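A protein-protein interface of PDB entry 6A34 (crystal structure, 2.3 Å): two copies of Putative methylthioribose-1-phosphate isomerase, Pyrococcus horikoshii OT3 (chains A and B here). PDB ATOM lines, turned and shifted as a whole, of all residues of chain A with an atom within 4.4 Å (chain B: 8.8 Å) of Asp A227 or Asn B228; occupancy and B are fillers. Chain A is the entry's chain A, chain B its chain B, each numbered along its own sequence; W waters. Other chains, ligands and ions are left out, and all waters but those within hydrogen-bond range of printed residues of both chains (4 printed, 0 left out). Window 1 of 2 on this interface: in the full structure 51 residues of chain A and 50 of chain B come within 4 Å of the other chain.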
ATOM      1  N   HIS A 166     -25.910  30.436  23.834  1.00  0.00           N
ATOM      2  CA  HIS A 166     -25.133  29.495  23.112  1.00  0.00           C
ATOM      3  C   HIS A 166     -24.307  28.688  24.111  1.00  0.00           C
ATOM      4  O   HIS A 166     -23.789  29.231  25.091  1.00  0.00           O
ATOM      5  CB  HIS A 166     -24.261  30.261  22.111  1.00  0.00           C
ATOM      6  CG  HIS A 166     -23.711  29.429  20.995  1.00  0.00           C
ATOM      7  ND1 HIS A 166     -24.462  29.080  19.902  1.00  0.00           N
ATOM      8  CD2 HIS A 166     -22.487  28.901  20.779  1.00  0.00           C
ATOM      9  CE1 HIS A 166     -23.727  28.367  19.060  1.00  0.00           C
ATOM     10  NE2 HIS A 166     -22.512  28.244  19.566  1.00  0.00           N
ATOM     11  N   ASP A 199     -29.399  27.633  21.722  1.00  0.00           N
ATOM     12  CA  ASP A 199     -28.763  26.952  20.599  1.00  0.00           C
ATOM     13  C   ASP A 199     -28.282  25.599  21.122  1.00  0.00           C
ATOM     14  O   ASP A 199     -27.624  25.552  22.163  1.00  0.00           O
ATOM     15  CB  ASP A 199     -27.566  27.736  20.060  1.00  0.00           C
ATOM     16  CG  ASP A 199     -27.877  29.066  19.386  1.00  0.00           C
ATOM     17  OD1 ASP A 199     -29.040  29.316  19.047  1.00  0.00           O
ATOM     18  OD2 ASP A 199     -26.924  29.846  19.188  1.00  0.00           O
ATOM     19  N   GLU A 200     -28.573  24.513  20.398  1.00  0.00           N
ATOM     20  CA  GLU A 200     -28.167  23.180  20.848  1.00  0.00           C
ATOM     21  C   GLU A 200     -26.641  23.092  20.974  1.00  0.00           C
ATOM     22  O   GLU A 200     -26.145  22.369  21.859  1.00  0.00           O
ATOM     23  CB  GLU A 200     -28.762  22.091  19.954  1.00  0.00           C
ATOM     24  CG  GLU A 200     -28.360  22.127  18.482  1.00  0.00           C
ATOM     25  CD  GLU A 200     -28.918  20.928  17.712  1.00  0.00           C
ATOM     26  OE1 GLU A 200     -29.635  20.137  18.359  1.00  0.00           O
ATOM     27  OE2 GLU A 200     -28.617  20.758  16.478  1.00  0.00           O
ATOM     28  N   THR A 201     -25.927  23.779  20.057  1.00  0.00           N
ATOM     29  CA  THR A 201     -24.465  23.965  20.035  1.00  0.00           C
ATOM     30  C   THR A 201     -23.700  22.686  19.660  1.00  0.00           C
ATOM     31  O   THR A 201     -22.962  22.084  20.472  1.00  0.00           O
ATOM     32  CB  THR A 201     -23.954  24.542  21.360  1.00  0.00           C
ATOM     33  OG1 THR A 201     -24.863  25.548  21.813  1.00  0.00           O
ATOM     34  CG2 THR A 201     -22.585  25.169  21.203  1.00  0.00           C
ATOM     35  N   ARG A 202     -23.845  22.301  18.393  1.00  0.00           N
ATOM     36  CA  ARG A 202     -23.046  21.271  17.775  1.00  0.00           C
ATOM     37  C   ARG A 202     -21.602  21.763  17.708  1.00  0.00           C
ATOM     38  O   ARG A 202     -21.373  22.968  17.676  1.00  0.00           O
ATOM     39  CB  ARG A 202     -23.554  20.952  16.360  1.00  0.00           C
ATOM     40  CG  ARG A 202     -24.709  19.958  16.303  1.00  0.00           C
ATOM     41  CD  ARG A 202     -24.305  18.527  16.623  1.00  0.00           C
ATOM     42  NE  ARG A 202     -23.513  17.921  15.571  1.00  0.00           N
ATOM     43  CZ  ARG A 202     -22.869  16.770  15.687  1.00  0.00           C
ATOM     44  NH1 ARG A 202     -22.771  16.181  16.872  1.00  0.00           N
ATOM     45  NH2 ARG A 202     -22.327  16.235  14.606  1.00  0.00           N
ATOM     46  N   ILE A 225     -33.301  25.118  20.063  1.00  0.00           N
ATOM     47  CA  ILE A 225     -33.292  25.205  18.586  1.00  0.00           C
ATOM     48  C   ILE A 225     -31.978  24.669  18.010  1.00  0.00           C
ATOM     49  O   ILE A 225     -30.906  24.689  18.662  1.00  0.00           O
ATOM     50  CB  ILE A 225     -33.478  26.650  18.097  1.00  0.00           C
ATOM     51  CG1 ILE A 225     -32.401  27.572  18.671  1.00  0.00           C
ATOM     52  CG2 ILE A 225     -34.892  27.186  18.343  1.00  0.00           C
ATOM     53  CD1 ILE A 225     -32.439  28.917  18.032  1.00  0.00           C
ATOM     54  N   ALA A 226     -32.048  24.274  16.734  1.00  0.00           N
ATOM     55  CA  ALA A 226     -30.854  23.954  15.957  1.00  0.00           C
ATOM     56  C   ALA A 226     -30.097  25.265  15.729  1.00  0.00           C
ATOM     57  O   ALA A 226     -30.696  26.316  15.598  1.00  0.00           O
ATOM     58  CB  ALA A 226     -31.208  23.276  14.646  1.00  0.00           C
ATOM     59  N   ASP A 227     -28.772  25.175  15.682  1.00  0.00           N
ATOM     60  CA  ASP A 227     -27.878  26.343  15.496  1.00  0.00           C
ATOM     61  C   ASP A 227     -28.267  27.136  14.249  1.00  0.00           C
ATOM     62  O   ASP A 227     -28.220  28.354  14.238  1.00  0.00           O
ATOM     63  CB  ASP A 227     -26.445  25.842  15.435  1.00  0.00           C
ATOM     64  CG  ASP A 227     -26.038  25.143  16.720  1.00  0.00           C
ATOM     65  OD1 ASP A 227     -26.365  25.701  17.803  1.00  0.00           O
ATOM     66  OD2 ASP A 227     -25.398  24.043  16.634  1.00  0.00           O
ATOM     67  N   ASN A 228     -28.601  26.396  13.191  1.00  0.00           N
ATOM     68  CA  ASN A 228     -29.101  26.903  11.939  1.00  0.00           C
ATOM     69  C   ASN A 228     -30.253  27.878  12.156  1.00  0.00           C
ATOM     70  O   ASN A 228     -30.492  28.739  11.332  1.00  0.00           O
ATOM     71  CB  ASN A 228     -29.607  25.770  11.022  1.00  0.00           C
ATOM     72  CG  ASN A 228     -28.502  25.152  10.196  1.00  0.00           C
ATOM     73  OD1 ASN A 228     -27.514  25.828   9.865  1.00  0.00           O
ATOM     74  ND2 ASN A 228     -28.666  23.890   9.850  1.00  0.00           N
ATOM     75  N   ALA A 229     -31.033  27.702  13.213  1.00  0.00           N
ATOM     76  CA  ALA A 229     -32.239  28.504  13.310  1.00  0.00           C
ATOM     77  C   ALA A 229     -31.991  29.821  14.048  1.00  0.00           C
ATOM     78  O   ALA A 229     -32.930  30.617  14.226  1.00  0.00           O
ATOM     79  CB  ALA A 229     -33.316  27.697  14.028  1.00  0.00           C
ATOM     80  N   ALA A 230     -30.789  30.058  14.577  1.00  0.00           N
ATOM     81  CA  ALA A 230     -30.660  31.288  15.422  1.00  0.00           C
ATOM     82  C   ALA A 230     -30.891  32.532  14.555  1.00  0.00           C
ATOM     83  O   ALA A 230     -31.474  33.509  14.989  1.00  0.00           O
ATOM     84  CB  ALA A 230     -29.331  31.320  16.130  1.00  0.00           C
ATOM     85  N   ILE A 259     -17.550  27.386  19.272  1.00  0.00           N
ATOM     86  CA  ILE A 259     -17.809  27.512  17.852  1.00  0.00           C
ATOM     87  C   ILE A 259     -19.287  27.850  17.619  1.00  0.00           C
ATOM     88  O   ILE A 259     -20.216  27.261  18.208  1.00  0.00           O
ATOM     89  CB  ILE A 259     -17.379  26.237  17.114  1.00  0.00           C
ATOM     90  CG1 ILE A 259     -17.358  26.433  15.601  1.00  0.00           C
ATOM     91  CG2 ILE A 259     -18.260  25.063  17.514  1.00  0.00           C
ATOM     92  CD1 ILE A 259     -16.209  27.283  15.112  1.00  0.00           C
ATOM     93  N   GLY A 260     -19.497  28.871  16.794  1.00  0.00           N
ATOM     94  CA  GLY A 260     -20.836  29.400  16.542  1.00  0.00           C
ATOM     95  C   GLY A 260     -21.057  30.790  17.107  1.00  0.00           C
ATOM     96  O   GLY A 260     -21.981  31.463  16.702  1.00  0.00           O
ATOM     97  N   MET A 263     -20.652  33.445  14.524  1.00  0.00           N
ATOM     98  CA  MET A 263     -21.869  33.413  13.666  1.00  0.00           C
ATOM     99  C   MET A 263     -22.976  34.298  14.260  1.00  0.00           C
ATOM    100  O   MET A 263     -23.602  35.107  13.542  1.00  0.00           O
ATOM    101  CB  MET A 263     -22.407  31.990  13.494  1.00  0.00           C
ATOM    102  CG  MET A 263     -23.766  31.947  12.734  1.00  0.00           C
ATOM    103  SD  MET A 263     -25.173  31.647  13.852  1.00  0.00           S
ATOM    104  CE  MET A 263     -24.811  29.914  14.120  1.00  0.00           C
ATOM    105  N   HIS B 166     -24.932  23.496   1.648  1.00  0.00           N
ATOM    106  CA  HIS B 166     -25.878  23.286   2.744  1.00  0.00           C
ATOM    107  C   HIS B 166     -26.982  22.317   2.269  1.00  0.00           C
ATOM    108  O   HIS B 166     -27.421  22.384   1.081  1.00  0.00           O
ATOM    109  CB  HIS B 166     -26.485  24.635   3.110  1.00  0.00           C
ATOM    110  CG  HIS B 166     -27.106  24.738   4.457  1.00  0.00           C
ATOM    111  ND1 HIS B 166     -26.350  24.802   5.606  1.00  0.00           N
ATOM    112  CD2 HIS B 166     -28.404  24.861   4.831  1.00  0.00           C
ATOM    113  CE1 HIS B 166     -27.158  24.946   6.647  1.00  0.00           C
ATOM    114  NE2 HIS B 166     -28.444  24.998   6.188  1.00  0.00           N
ATOM    115  N   ASP B 199     -22.008  21.833   5.080  1.00  0.00           N
ATOM    116  CA  ASP B 199     -22.691  21.954   6.359  1.00  0.00           C
ATOM    117  C   ASP B 199     -23.486  20.642   6.600  1.00  0.00           C
ATOM    118  O   ASP B 199     -24.281  20.172   5.715  1.00  0.00           O
ATOM    119  CB  ASP B 199     -23.613  23.183   6.377  1.00  0.00           C
ATOM    120  CG  ASP B 199     -22.993  24.566   6.211  1.00  0.00           C
ATOM    121  OD1 ASP B 199     -21.754  24.694   6.245  1.00  0.00           O
ATOM    122  OD2 ASP B 199     -23.780  25.531   6.028  1.00  0.00           O
ATOM    123  N   GLU B 200     -23.308  20.031   7.779  1.00  0.00           N
ATOM    124  CA  GLU B 200     -24.088  18.812   8.139  1.00  0.00           C
ATOM    125  C   GLU B 200     -25.600  19.114   8.121  1.00  0.00           C
ATOM    126  O   GLU B 200     -26.389  18.236   7.835  1.00  0.00           O
ATOM    127  CB  GLU B 200     -23.613  18.227   9.470  1.00  0.00           C
ATOM    128  CG  GLU B 200     -23.849  19.122  10.675  1.00  0.00           C
ATOM    129  CD  GLU B 200     -23.565  18.471  12.030  1.00  0.00           C
ATOM    130  OE1 GLU B 200     -22.943  17.391  12.048  1.00  0.00           O
ATOM    131  OE2 GLU B 200     -23.972  19.066  13.077  1.00  0.00           O
ATOM    132  N   THR B 201     -25.997  20.351   8.452  1.00  0.00           N
ATOM    133  CA  THR B 201     -27.391  20.841   8.326  1.00  0.00           C
ATOM    134  C   THR B 201     -28.331  20.129   9.314  1.00  0.00           C
ATOM    135  O   THR B 201     -29.222  19.320   8.918  1.00  0.00           O
ATOM    136  CB  THR B 201     -27.927  20.658   6.894  1.00  0.00           C
ATOM    137  OG1 THR B 201     -26.913  21.114   5.994  1.00  0.00           O
ATOM    138  CG2 THR B 201     -29.217  21.408   6.648  1.00  0.00           C
ATOM    139  N   ARG B 202     -28.131  20.419  10.602  1.00  0.00           N
ATOM    140  CA  ARG B 202     -29.098  20.071  11.615  1.00  0.00           C
ATOM    141  C   ARG B 202     -30.389  20.806  11.271  1.00  0.00           C
ATOM    142  O   ARG B 202     -30.362  21.858  10.621  1.00  0.00           O
ATOM    143  CB  ARG B 202     -28.581  20.397  13.020  1.00  0.00           C
ATOM    144  CG  ARG B 202     -27.664  19.332  13.611  1.00  0.00           C
ATOM    145  CD  ARG B 202     -28.408  18.081  14.107  1.00  0.00           C
ATOM    146  NE  ARG B 202     -29.274  18.413  15.241  1.00  0.00           N
ATOM    147  CZ  ARG B 202     -30.190  17.605  15.798  1.00  0.00           C
ATOM    148  NH1 ARG B 202     -30.566  16.488  15.183  1.00  0.00           N
ATOM    149  NH2 ARG B 202     -30.702  17.923  16.983  1.00  0.00           N
ATOM    150  N   PRO B 203     -31.520  20.260  11.740  1.00  0.00           N
ATOM    151  CA  PRO B 203     -31.587  19.077  12.592  1.00  0.00           C
ATOM    152  C   PRO B 203     -31.645  17.714  11.874  1.00  0.00           C
ATOM    153  O   PRO B 203     -31.286  16.666  12.466  1.00  0.00           O
ATOM    154  CB  PRO B 203     -32.882  19.253  13.386  1.00  0.00           C
ATOM    155  CG  PRO B 203     -33.682  20.225  12.578  1.00  0.00           C
ATOM    156  CD  PRO B 203     -32.671  21.122  11.904  1.00  0.00           C
ATOM    157  N   ILE B 225     -18.525  19.846   8.218  1.00  0.00           N
ATOM    158  CA  ILE B 225     -18.467  20.739   9.377  1.00  0.00           C
ATOM    159  C   ILE B 225     -19.841  20.875  10.027  1.00  0.00           C
ATOM    160  O   ILE B 225     -20.892  20.789   9.378  1.00  0.00           O
ATOM    161  CB  ILE B 225     -17.943  22.133   8.989  1.00  0.00           C
ATOM    162  CG1 ILE B 225     -18.852  22.843   7.989  1.00  0.00           C
ATOM    163  CG2 ILE B 225     -16.520  22.055   8.477  1.00  0.00           C
ATOM    164  CD1 ILE B 225     -18.366  24.230   7.606  1.00  0.00           C
ATOM    165  N   ALA B 226     -19.806  21.151  11.334  1.00  0.00           N
ATOM    166  CA  ALA B 226     -20.933  21.649  12.053  1.00  0.00           C
ATOM    167  C   ALA B 226     -21.348  23.005  11.457  1.00  0.00           C
ATOM    168  O   ALA B 226     -20.503  23.752  10.966  1.00  0.00           O
ATOM    169  CB  ALA B 226     -20.572  21.759  13.511  1.00  0.00           C
ATOM    170  N   ASP B 227     -22.662  23.293  11.499  1.00  0.00           N
ATOM    171  CA  ASP B 227     -23.265  24.469  10.908  1.00  0.00           C
ATOM    172  C   ASP B 227     -22.638  25.718  11.549  1.00  0.00           C
ATOM    173  O   ASP B 227     -22.501  26.756  10.902  1.00  0.00           O
ATOM    174  CB  ASP B 227     -24.805  24.424  11.017  1.00  0.00           C
ATOM    175  CG  ASP B 227     -25.431  23.196  10.328  1.00  0.00           C
ATOM    176  OD1 ASP B 227     -24.996  22.869   9.184  1.00  0.00           O
ATOM    177  OD2 ASP B 227     -26.307  22.536  10.944  1.00  0.00           O
ATOM    178  N   ASN B 228     -22.315  25.608  12.842  1.00  0.00           N
ATOM    179  CA  ASN B 228     -21.732  26.684  13.652  1.00  0.00           C
ATOM    180  C   ASN B 228     -20.385  27.134  13.078  1.00  0.00           C
ATOM    181  O   ASN B 228     -19.983  28.234  13.305  1.00  0.00           O
ATOM    182  CB  ASN B 228     -21.466  26.209  15.083  1.00  0.00           C
ATOM    183  CG  ASN B 228     -22.651  26.365  16.001  1.00  0.00           C
ATOM    184  OD1 ASN B 228     -23.453  27.283  15.835  1.00  0.00           O
ATOM    185  ND2 ASN B 228     -22.761  25.481  16.965  1.00  0.00           N
ATOM    186  N   ALA B 229     -19.684  26.226  12.399  1.00  0.00           N
ATOM    187  CA  ALA B 229     -18.357  26.475  11.858  1.00  0.00           C
ATOM    188  C   ALA B 229     -18.381  27.144  10.467  1.00  0.00           C
ATOM    189  O   ALA B 229     -17.341  27.586   9.978  1.00  0.00           O
ATOM    190  CB  ALA B 229     -17.587  25.184  11.853  1.00  0.00           C
ATOM    191  N   ALA B 230     -19.541  27.282   9.820  1.00  0.00           N
ATOM    192  CA  ALA B 230     -19.552  27.924   8.500  1.00  0.00           C
ATOM    193  C   ALA B 230     -18.962  29.337   8.596  1.00  0.00           C
ATOM    194  O   ALA B 230     -18.166  29.750   7.736  1.00  0.00           O
ATOM    195  CB  ALA B 230     -20.938  27.980   7.911  1.00  0.00           C
ATOM    196  N   ALA B 231     -19.436  30.104   9.585  1.00  0.00           N
ATOM    197  CA  ALA B 231     -19.046  31.487   9.728  1.00  0.00           C
ATOM    198  C   ALA B 231     -17.520  31.571   9.846  1.00  0.00           C
ATOM    199  O   ALA B 231     -16.868  32.383   9.217  1.00  0.00           O
ATOM    200  CB  ALA B 231     -19.731  32.115  10.905  1.00  0.00           C
ATOM    201  N   PHE B 232     -16.971  30.657  10.636  1.00  0.00           N
ATOM    202  CA  PHE B 232     -15.615  30.648  10.985  1.00  0.00           C
ATOM    203  C   PHE B 232     -14.769  30.302   9.763  1.00  0.00           C
ATOM    204  O   PHE B 232     -13.732  30.904   9.597  1.00  0.00           O
ATOM    205  CB  PHE B 232     -15.378  29.664  12.132  1.00  0.00           C
ATOM    206  CG  PHE B 232     -13.930  29.469  12.497  1.00  0.00           C
ATOM    207  CD1 PHE B 232     -13.300  30.331  13.381  1.00  0.00           C
ATOM    208  CD2 PHE B 232     -13.175  28.463  11.895  1.00  0.00           C
ATOM    209  CE1 PHE B 232     -11.959  30.153  13.715  1.00  0.00           C
ATOM    210  CE2 PHE B 232     -11.831  28.290  12.214  1.00  0.00           C
ATOM    211  CZ  PHE B 232     -11.235  29.119  13.155  1.00  0.00           C
ATOM    212  N   VAL B 233     -15.187  29.318   8.947  1.00  0.00           N
ATOM    213  CA  VAL B 233     -14.364  28.930   7.774  1.00  0.00           C
ATOM    214  C   VAL B 233     -14.409  30.077   6.761  1.00  0.00           C
ATOM    215  O   VAL B 233     -13.397  30.298   6.084  1.00  0.00           O
ATOM    216  CB  VAL B 233     -14.699  27.571   7.117  1.00  0.00           C
ATOM    217  CG1 VAL B 233     -14.530  26.416   8.077  1.00  0.00           C
ATOM    218  CG2 VAL B 233     -16.075  27.554   6.488  1.00  0.00           C
ATOM    219  N   MET B 234     -15.535  30.809   6.690  1.00  0.00           N
ATOM    220  CA  MET B 234     -15.591  32.026   5.891  1.00  0.00           C
ATOM    221  C   MET B 234     -14.593  33.060   6.436  1.00  0.00           C
ATOM    222  O   MET B 234     -13.852  33.612   5.656  1.00  0.00           O
ATOM    223  CB  MET B 234     -16.984  32.645   5.829  1.00  0.00           C
ATOM    224  CG  MET B 234     -17.981  31.790   5.063  1.00  0.00           C
ATOM    225  SD  MET B 234     -19.570  32.562   5.055  1.00  0.00           S
ATOM    226  CE  MET B 234     -20.705  31.180   5.258  1.00  0.00           C
ATOM    227  N   ILE B 259     -33.391  25.381   6.644  1.00  0.00           N
ATOM    228  CA  ILE B 259     -33.031  26.202   7.773  1.00  0.00           C
ATOM    229  C   ILE B 259     -31.504  26.282   7.844  1.00  0.00           C
ATOM    230  O   ILE B 259     -30.800  25.290   7.674  1.00  0.00           O
ATOM    231  CB  ILE B 259     -33.665  25.649   9.066  1.00  0.00           C
ATOM    232  CG1 ILE B 259     -33.523  26.634  10.228  1.00  0.00           C
ATOM    233  CG2 ILE B 259     -33.117  24.276   9.402  1.00  0.00           C
ATOM    234  CD1 ILE B 259     -34.297  27.926  10.022  1.00  0.00           C
ATOM    235  N   GLY B 260     -31.011  27.514   7.991  1.00  0.00           N
ATOM    236  CA  GLY B 260     -29.593  27.793   7.996  1.00  0.00           C
ATOM    237  C   GLY B 260     -29.116  28.544   6.764  1.00  0.00           C
ATOM    238  O   GLY B 260     -28.043  29.198   6.821  1.00  0.00           O
ATOM    239  N   THR B 261     -29.873  28.444   5.665  1.00  0.00           N
ATOM    240  CA  THR B 261     -29.549  29.086   4.375  1.00  0.00           C
ATOM    241  C   THR B 261     -29.436  30.606   4.571  1.00  0.00           C
ATOM    242  O   THR B 261     -28.510  31.233   4.100  1.00  0.00           O
ATOM    243  CB  THR B 261     -30.574  28.774   3.271  1.00  0.00           C
ATOM    244  OG1 THR B 261     -30.648  27.358   2.997  1.00  0.00           O
ATOM    245  CG2 THR B 261     -30.266  29.543   2.005  1.00  0.00           C
ATOM    246  N   MET B 263     -28.803  32.165   7.377  1.00  0.00           N
ATOM    247  CA  MET B 263     -27.558  32.316   8.116  1.00  0.00           C
ATOM    248  C   MET B 263     -26.363  32.388   7.147  1.00  0.00           C
ATOM    249  O   MET B 263     -25.506  33.283   7.249  1.00  0.00           O
ATOM    250  CB  MET B 263     -27.360  31.177   9.112  1.00  0.00           C
ATOM    251  CG  MET B 263     -26.100  31.329   9.937  1.00  0.00           C
ATOM    252  SD  MET B 263     -24.815  30.266   9.296  1.00  0.00           S
ATOM    253  CE  MET B 263     -25.417  28.707   9.931  1.00  0.00           C
ATOM    254  N   LEU B 264     -26.295  31.469   6.200  1.00  0.00           N
ATOM    255  CA  LEU B 264     -25.188  31.505   5.242  1.00  0.00           C
ATOM    256  C   LEU B 264     -25.208  32.792   4.422  1.00  0.00           C
ATOM    257  O   LEU B 264     -24.171  33.379   4.184  1.00  0.00           O
ATOM    258  CB  LEU B 264     -25.267  30.316   4.303  1.00  0.00           C
ATOM    259  CG  LEU B 264     -24.904  28.989   4.933  1.00  0.00           C
ATOM    260  CD1 LEU B 264     -25.085  27.854   3.935  1.00  0.00           C
ATOM    261  CD2 LEU B 264     -23.501  29.027   5.454  1.00  0.00           C
ATOM    262  N   LEU B 267     -23.750  35.607   6.410  1.00  0.00           N
ATOM    263  CA  LEU B 267     -22.317  35.486   6.570  1.00  0.00           C
ATOM    264  C   LEU B 267     -21.563  35.705   5.266  1.00  0.00           C
ATOM    265  O   LEU B 267     -20.444  36.254   5.325  1.00  0.00           O
ATOM    266  CB  LEU B 267     -21.954  34.131   7.142  1.00  0.00           C
ATOM    267  CG  LEU B 267     -22.530  33.916   8.527  1.00  0.00           C
ATOM    268  CD1 LEU B 267     -22.467  32.431   8.849  1.00  0.00           C
ATOM    269  CD2 LEU B 267     -21.788  34.760   9.543  1.00  0.00           C
ATOM    270  N   VAL B 304     -35.192  17.646  16.797  1.00  0.00           N
ATOM    271  CA  VAL B 304     -34.204  18.446  17.558  1.00  0.00           C
ATOM    272  C   VAL B 304     -33.782  17.699  18.825  1.00  0.00           C
ATOM    273  O   VAL B 304     -32.635  17.721  19.204  1.00  0.00           O
ATOM    274  CB  VAL B 304     -34.745  19.835  17.926  1.00  0.00           C
ATOM    275  CG1 VAL B 304     -33.766  20.604  18.803  1.00  0.00           C
ATOM    276  CG2 VAL B 304     -35.069  20.632  16.683  1.00  0.00           C
ATOM    277  N   TYR B 319     -38.357  24.769  19.082  1.00  0.00           N
ATOM    278  CA  TYR B 319     -38.809  25.391  17.859  1.00  0.00           C
ATOM    279  C   TYR B 319     -37.994  24.775  16.708  1.00  0.00           C
ATOM    280  O   TYR B 319     -36.722  24.761  16.733  1.00  0.00           O
ATOM    281  CB  TYR B 319     -38.655  26.905  18.010  1.00  0.00           C
ATOM    282  CG  TYR B 319     -39.184  27.759  16.887  1.00  0.00           C
ATOM    283  CD1 TYR B 319     -40.507  27.642  16.483  1.00  0.00           C
ATOM    284  CD2 TYR B 319     -38.401  28.722  16.267  1.00  0.00           C
ATOM    285  CE1 TYR B 319     -41.035  28.432  15.470  1.00  0.00           C
ATOM    286  CE2 TYR B 319     -38.920  29.526  15.257  1.00  0.00           C
ATOM    287  CZ  TYR B 319     -40.243  29.386  14.859  1.00  0.00           C
ATOM    288  OH  TYR B 319     -40.802  30.136  13.865  1.00  0.00           O
ATOM    289  N   ASP B 324     -36.075  28.548   6.002  1.00  0.00           N
ATOM    290  CA  ASP B 324     -36.065  29.989   6.176  1.00  0.00           C
ATOM    291  C   ASP B 324     -36.200  30.641   4.799  1.00  0.00           C
ATOM    292  O   ASP B 324     -36.247  29.970   3.785  1.00  0.00           O
ATOM    293  CB  ASP B 324     -34.878  30.486   7.018  1.00  0.00           C
ATOM    294  CG  ASP B 324     -33.496  30.093   6.529  1.00  0.00           C
ATOM    295  OD1 ASP B 324     -33.306  30.004   5.311  1.00  0.00           O
ATOM    296  OD2 ASP B 324     -32.616  29.887   7.393  1.00  0.00           O
HETATM  297  O   HOH W   1     -34.422  24.445  15.289  1.00  0.00           O
HETATM  298  O   HOH W   2     -27.769  23.758  12.916  1.00  0.00           O
HETATM  299  O   HOH W   3     -31.407  30.767   9.474  1.00  0.00           O
HETATM  300  O   HOH W   4     -23.839  23.774  14.532  1.00  0.00           O
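ND2 of Asn A228 is in hydrogen-bond range of O of Ile B259 (3.4 Å). NE of Arg B202 lies within salt-bridge range of OE2 of Glu A200 (2.7 Å). The backbone carbonyl oxygen (O) of Ile A259 is in hydrogen-bond range of the side-chain amide nitrogen (ND2) of Asn B228, at 3.3 Å. The side-chain amide nitrogen (ND2) of Asn A228 is in hydrogen-bond range of the backbone carbonyl oxygen (O) of Arg B202. ND2 of Asn B228 is in hydrogen-bond range of O of Arg A202 (3.0 Å). ND2 of Asn A228 is in hydrogen-bond range of OD2 of Asp B227 (2.9 Å). The side-chain carboxylate (OE2) of Glu B200 is in salt-bridge range of the guanidinium group (NE) of Arg A202 (2.8 Å). The side-chain carboxylate of Asp A227 is in hydrogen-bond range of the side-chain amide nitrogen of Asn B228, at 3.0 Å.
OD2 of Asp B227 sits at hydrogen-bond distance from N of Arg B202 (2.8 Å). The backbone NH (N) of Thr B201 sits at hydrogen-bond distance from the side-chain carboxylate (OD1) of Asp B227, at 2.8 Å. The backbone NH of Thr A201 lies within hydrogen-bond range of the side-chain carboxylate of Asp A227, at 3.0 Å. The backbone carbonyl oxygen of Asp A199 is in hydrogen-bond range of the side-chain hydroxyl of Thr A201, at 2.8 Å.
Asn B228 touches His A166. CA of Thr A201 touches ND2 of Asn B228, at 3.8 Å. Ile A225 touches Tyr B319 (CG2 to O, 3.4 Å). Pro B203 touches Ala A226. OD1 of Asn A228 touches CE1 of His B166, at 3.4 Å. Asn A228 touches Thr B201 (ND2 to CA, 3.6 Å). Gly B260 touches Asn A228 (CA to OD1, 3.4 Å). Asn A228 touches Met B263 (OD1 to CE, 3.6 Å). CG1 of Ile A259 touches CA of Ala B229 (3.9 Å). Met A263 touches Ala B231 (CA to CB, 3.7 Å).
Asp A227 touches just one residue of chain B: Asn B228 (3.0 Å). Asn B228 touches just these residues of chain A: His A166, Thr A201, Arg A202, Asp A227, Ile A259, Gly A260 and Met A263. Of chain B, only Pro B203 comes within 4 Å of Ala A226. Gly A260 touches just one residue of chain B: Asn B228. Of the printed residues of chain B, His A166 touches Asn B228 (3.4 Å). Printed residues of chain B within 4 Å of Asn A228: His B166, Thr B201, Arg B202, Asp B227, Ile B259, Gly B260 and Met B263. Of the printed residues of chain B, Ile A259 touches Asn B228 (3.3 Å), Ala B229 (3.9 Å) and Phe B232 (3.9 Å). Of the printed residues of chain B, Ile A225 touches Tyr B319 (3.4 Å). Ala A230 touches none of the printed residues of chain B. The nearest residue of chain B that does not touch Asp A227 is Asp B227 (4.9 Å). The nearest printed residue of chain A that does not touch Asn B228 is Asp A199 (5.5 Å).
Printed residues of chain A that touch a printed residue of chain B: His A166, Glu A200, Thr A201, Arg A202, Ile A225, Ala A226, Asp A227, Asn A228, Ala A229, Ile A259, Gly A260 and Met A263. Of the 25 printed residues of chain B, 15 touch a printed residue of chain A. Hydrophobic or aromatic side chains of chain B within 4 Å of the printed part of chain A: His B166, Pro B203, Ala B229, Ala B231, Phe B232, Ile B259, Met B263 and Tyr B319.
His A166 touches Asn B228, and with the chains exchanged Asn A228 touches His B166. Arg A202 touches Asn B228, and with the chains exchanged Asn A228 touches Arg B202. Asp A227 touches Asn B228, and with the chains exchanged Asn A228 touches Asp B227. Asn A228 touches Gly B260, and with the chains exchanged Gly A260 touches Asn B228.
Water W3 lies within hydrogen-bond range of OD2 of Asp B324 (2.6 Å) and O of Asn A228 (2.9 Å). Water W2 lies within hydrogen-bond range of the side-chain carboxylate (OD2) of Asp B227 (2.7 Å), the backbone NH (N) of Asn A228 (2.8 Å) and the backbone NH (N) of Asp A227 (3.3 Å).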
